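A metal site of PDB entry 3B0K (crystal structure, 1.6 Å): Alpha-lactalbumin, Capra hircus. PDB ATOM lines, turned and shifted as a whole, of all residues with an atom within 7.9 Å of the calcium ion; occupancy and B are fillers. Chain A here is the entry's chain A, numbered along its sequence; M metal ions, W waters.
Water W1 bridges OD2 of Asp 87 (2.6 Å) and OD2 of Asp 82 (2.6 Å).
The calcium ion is bound by O of Asp 84 (2.3 Å). OD1 of Asp 82 is bound to the calcium ion, at 2.3 Å. The backbone carbonyl oxygen (O) of Lys 79 binds the calcium ion (2.3 Å). OD1 of Asp 87 binds the calcium ion. The calcium ion is bound by OD1 of Asp 88 (2.4 Å). The calcium ion is bound by water W2 (2.5 Å). Water W1 is bound to the calcium ion, 2.5 Å away. The calcium ion has seven donor atoms within binding distance.
The backbone carbonyl oxygen (O) of Asp 82 is in hydrogen-bond range of the side-chain hydroxyl (OG1) of Thr 38 (3.3 Å). OG1 of Thr 86 sits at hydrogen-bond distance from OD1 of Asp 84.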
ATOM      1  N   THR A  38       8.509  -4.606  -4.585  1.00  0.00           N
ATOM      2  CA  THR A  38       9.816  -5.253  -4.236  1.00  0.00           C
ATOM      3  C   THR A  38      10.885  -4.304  -3.610  1.00  0.00           C
ATOM      4  O   THR A  38      11.827  -4.732  -2.959  1.00  0.00           O
ATOM      5  CB  THR A  38      10.468  -6.042  -5.411  1.00  0.00           C
ATOM      6  OG1 THR A  38      11.043  -5.081  -6.327  1.00  0.00           O
ATOM      7  CG2 THR A  38       9.473  -7.068  -5.984  1.00  0.00           C
ATOM      8  N   GLY A  51      11.638  -4.870   1.389  1.00  0.00           N
ATOM      9  CA  GLY A  51      11.159  -5.684   0.297  1.00  0.00           C
ATOM     10  C   GLY A  51       9.718  -6.135   0.353  1.00  0.00           C
ATOM     11  O   GLY A  51       8.935  -5.709   1.226  1.00  0.00           O
ATOM     12  N   ILE A  75      22.294 -12.477   5.268  1.00  0.00           N
ATOM     13  CA  ILE A  75      22.286 -11.716   4.032  1.00  0.00           C
ATOM     14  C   ILE A  75      22.150 -10.223   4.331  1.00  0.00           C
ATOM     15  O   ILE A  75      21.582  -9.850   5.363  1.00  0.00           O
ATOM     16  CB  ILE A  75      21.110 -12.219   3.190  1.00  0.00           C
ATOM     17  CG1 ILE A  75      21.110 -11.685   1.761  1.00  0.00           C
ATOM     18  CG2 ILE A  75      19.759 -11.889   3.798  1.00  0.00           C
ATOM     19  CD1 ILE A  75      20.238 -12.518   0.843  1.00  0.00           C
ATOM     20  N   SER A  76      22.712  -9.379   3.481  1.00  0.00           N
ATOM     21  CA  SER A  76      22.475  -7.949   3.527  1.00  0.00           C
ATOM     22  C   SER A  76      21.053  -7.670   3.105  1.00  0.00           C
ATOM     23  O   SER A  76      20.546  -8.210   2.121  1.00  0.00           O
ATOM     24  CB  SER A  76      23.400  -7.151   2.639  1.00  0.00           C
ATOM     25  OG  SER A  76      23.430  -7.622   1.324  1.00  0.00           O
ATOM     26  N   CYS A  77      20.391  -6.893   3.936  1.00  0.00           N
ATOM     27  CA  CYS A  77      18.994  -6.493   3.666  1.00  0.00           C
ATOM     28  C   CYS A  77      18.743  -5.935   2.284  1.00  0.00           C
ATOM     29  O   CYS A  77      17.633  -6.119   1.726  1.00  0.00           O
ATOM     30  CB  CYS A  77      18.449  -5.538   4.716  1.00  0.00           C
ATOM     31  SG  CYS A  77      18.508  -6.055   6.434  1.00  0.00           S
ATOM     32  N   ASP A  78      19.699  -5.217   1.712  1.00  0.00           N
ATOM     33  CA  ASP A  78      19.440  -4.616   0.430  1.00  0.00           C
ATOM     34  C   ASP A  78      19.262  -5.643  -0.692  1.00  0.00           C
ATOM     35  O   ASP A  78      18.700  -5.297  -1.768  1.00  0.00           O
ATOM     36  CB  ASP A  78      20.451  -3.489   0.140  1.00  0.00           C
ATOM     37  CG  ASP A  78      21.888  -3.957   0.018  1.00  0.00           C
ATOM     38  OD1 ASP A  78      22.210  -5.165   0.247  1.00  0.00           O
ATOM     39  OD2 ASP A  78      22.708  -3.010  -0.211  1.00  0.00           O
ATOM     40  N   LYS A  79      19.601  -6.913  -0.464  1.00  0.00           N
ATOM     41  CA  LYS A  79      19.323  -7.945  -1.435  1.00  0.00           C
ATOM     42  C   LYS A  79      17.806  -8.212  -1.514  1.00  0.00           C
ATOM     43  O   LYS A  79      17.343  -8.818  -2.496  1.00  0.00           O
ATOM     44  CB  LYS A  79      20.059  -9.216  -1.117  1.00  0.00           C
ATOM     45  CG  LYS A  79      21.582  -9.089  -1.171  1.00  0.00           C
ATOM     46  CD  LYS A  79      21.964  -9.004  -2.570  1.00  0.00           C
ATOM     47  CE  LYS A  79      23.420  -9.410  -2.779  1.00  0.00           C
ATOM     48  NZ  LYS A  79      23.655  -9.248  -4.241  1.00  0.00           N
ATOM     49  N   PHE A  80      17.033  -7.663  -0.571  1.00  0.00           N
ATOM     50  CA  PHE A  80      15.575  -7.763  -0.647  1.00  0.00           C
ATOM     51  C   PHE A  80      14.931  -6.551  -1.338  1.00  0.00           C
ATOM     52  O   PHE A  80      13.689  -6.352  -1.219  1.00  0.00           O
ATOM     53  CB  PHE A  80      15.049  -7.917   0.770  1.00  0.00           C
ATOM     54  CG  PHE A  80      15.564  -9.104   1.512  1.00  0.00           C
ATOM     55  CD1 PHE A  80      15.759 -10.315   0.890  1.00  0.00           C
ATOM     56  CD2 PHE A  80      15.848  -9.036   2.902  1.00  0.00           C
ATOM     57  CE1 PHE A  80      16.227 -11.449   1.534  1.00  0.00           C
ATOM     58  CE2 PHE A  80      16.286 -10.169   3.563  1.00  0.00           C
ATOM     59  CZ  PHE A  80      16.409 -11.390   2.910  1.00  0.00           C
ATOM     60  N   LEU A  81      15.742  -5.708  -1.962  1.00  0.00           N
ATOM     61  CA  LEU A  81      15.211  -4.511  -2.672  1.00  0.00           C
ATOM     62  C   LEU A  81      15.337  -4.634  -4.158  1.00  0.00           C
ATOM     63  O   LEU A  81      14.936  -3.711  -4.892  1.00  0.00           O
ATOM     64  CB  LEU A  81      15.848  -3.227  -2.149  1.00  0.00           C
ATOM     65  CG  LEU A  81      15.634  -2.968  -0.675  1.00  0.00           C
ATOM     66  CD1 LEU A  81      16.441  -1.745  -0.268  1.00  0.00           C
ATOM     67  CD2 LEU A  81      14.208  -2.785  -0.387  1.00  0.00           C
ATOM     68  N   ASP A  82      15.857  -5.761  -4.598  1.00  0.00           N
ATOM     69  CA  ASP A  82      16.059  -5.931  -6.064  1.00  0.00           C
ATOM     70  C   ASP A  82      14.870  -6.670  -6.680  1.00  0.00           C
ATOM     71  O   ASP A  82      13.822  -6.884  -6.020  1.00  0.00           O
ATOM     72  CB  ASP A  82      17.425  -6.574  -6.357  1.00  0.00           C
ATOM     73  CG  ASP A  82      17.554  -8.031  -5.845  1.00  0.00           C
ATOM     74  OD1 ASP A  82      16.505  -8.686  -5.498  1.00  0.00           O
ATOM     75  OD2 ASP A  82      18.731  -8.564  -5.941  1.00  0.00           O
ATOM     76  N   ASP A  83      14.964  -6.988  -7.975  1.00  0.00           N
ATOM     77  CA  ASP A  83      13.803  -7.630  -8.618  1.00  0.00           C
ATOM     78  C   ASP A  83      13.822  -9.159  -8.620  1.00  0.00           C
ATOM     79  O   ASP A  83      12.895  -9.764  -9.216  1.00  0.00           O
ATOM     80  CB  ASP A  83      13.759  -7.065 -10.056  1.00  0.00           C
ATOM     81  CG  ASP A  83      13.426  -5.597 -10.065  1.00  0.00           C
ATOM     82  OD1 ASP A  83      12.918  -5.079  -9.066  1.00  0.00           O
ATOM     83  OD2 ASP A  83      13.595  -4.970 -11.114  1.00  0.00           O
ATOM     84  N   ASP A  84      14.814  -9.783  -7.985  1.00  0.00           N
ATOM     85  CA  ASP A  84      14.890 -11.244  -7.913  1.00  0.00           C
ATOM     86  C   ASP A  84      14.452 -11.694  -6.581  1.00  0.00           C
ATOM     87  O   ASP A  84      15.118 -11.413  -5.582  1.00  0.00           O
ATOM     88  CB  ASP A  84      16.354 -11.672  -8.096  1.00  0.00           C
ATOM     89  CG  ASP A  84      16.526 -13.146  -8.160  1.00  0.00           C
ATOM     90  OD1 ASP A  84      15.574 -13.913  -7.938  1.00  0.00           O
ATOM     91  OD2 ASP A  84      17.665 -13.590  -8.478  1.00  0.00           O
ATOM     92  N   LEU A  85      13.307 -12.339  -6.542  1.00  0.00           N
ATOM     93  CA  LEU A  85      12.771 -12.771  -5.218  1.00  0.00           C
ATOM     94  C   LEU A  85      13.294 -14.142  -4.731  1.00  0.00           C
ATOM     95  O   LEU A  85      12.802 -14.605  -3.676  1.00  0.00           O
ATOM     96  CB  LEU A  85      11.261 -12.782  -5.322  1.00  0.00           C
ATOM     97  CG  LEU A  85      10.609 -11.424  -5.569  1.00  0.00           C
ATOM     98  CD1 LEU A  85       9.088 -11.612  -5.693  1.00  0.00           C
ATOM     99  CD2 LEU A  85      10.849 -10.403  -4.431  1.00  0.00           C
ATOM    100  N   THR A  86      14.240 -14.800  -5.399  1.00  0.00           N
ATOM    101  CA  THR A  86      14.801 -16.055  -4.934  1.00  0.00           C
ATOM    102  C   THR A  86      15.289 -15.939  -3.457  1.00  0.00           C
ATOM    103  O   THR A  86      14.884 -16.766  -2.636  1.00  0.00           O
ATOM    104  CB  THR A  86      15.912 -16.488  -5.862  1.00  0.00           C
ATOM    105  OG1 THR A  86      15.391 -16.522  -7.191  1.00  0.00           O
ATOM    106  CG2 THR A  86      16.415 -17.885  -5.466  1.00  0.00           C
ATOM    107  N   ASP A  87      16.130 -14.923  -3.163  1.00  0.00           N
ATOM    108  CA  ASP A  87      16.637 -14.829  -1.792  1.00  0.00           C
ATOM    109  C   ASP A  87      15.538 -14.392  -0.831  1.00  0.00           C
ATOM    110  O   ASP A  87      15.491 -14.862   0.338  1.00  0.00           O
ATOM    111  CB  ASP A  87      17.961 -14.014  -1.679  1.00  0.00           C
ATOM    112  CG  ASP A  87      17.925 -12.650  -2.396  1.00  0.00           C
ATOM    113  OD1 ASP A  87      16.789 -12.118  -2.635  1.00  0.00           O
ATOM    114  OD2 ASP A  87      19.033 -12.090  -2.633  1.00  0.00           O
ATOM    115  N   ASP A  88      14.681 -13.445  -1.214  1.00  0.00           N
ATOM    116  CA  ASP A  88      13.534 -13.087  -0.379  1.00  0.00           C
ATOM    117  C   ASP A  88      12.753 -14.305   0.063  1.00  0.00           C
ATOM    118  O   ASP A  88      12.391 -14.456   1.233  1.00  0.00           O
ATOM    119  CB  ASP A  88      12.604 -12.145  -1.122  1.00  0.00           C
ATOM    120  CG  ASP A  88      13.261 -10.836  -1.612  1.00  0.00           C
ATOM    121  OD1 ASP A  88      14.225 -10.961  -2.397  1.00  0.00           O
ATOM    122  OD2 ASP A  88      12.861  -9.732  -1.193  1.00  0.00           O
ATOM    123  N   ILE A  89      12.566 -15.256  -0.848  1.00  0.00           N
ATOM    124  CA  ILE A  89      11.738 -16.476  -0.638  1.00  0.00           C
ATOM    125  C   ILE A  89      12.469 -17.427   0.316  1.00  0.00           C
ATOM    126  O   ILE A  89      11.866 -17.955   1.261  1.00  0.00           O
ATOM    127  CB  ILE A  89      11.402 -17.170  -1.965  1.00  0.00           C
ATOM    128  CG1 ILE A  89      10.349 -16.331  -2.683  1.00  0.00           C
ATOM    129  CG2 ILE A  89      10.946 -18.615  -1.697  1.00  0.00           C
ATOM    130  CD1 ILE A  89      10.173 -16.789  -4.093  1.00  0.00           C
HETATM  131 CA    CA M   1      16.008 -10.209  -3.829  1.00  0.00          CA
HETATM  132  O   HOH W   1      18.266 -10.849  -4.775  1.00  0.00           O
HETATM  133  O   HOH W   2      14.230  -8.513  -3.821  1.00  0.00           O
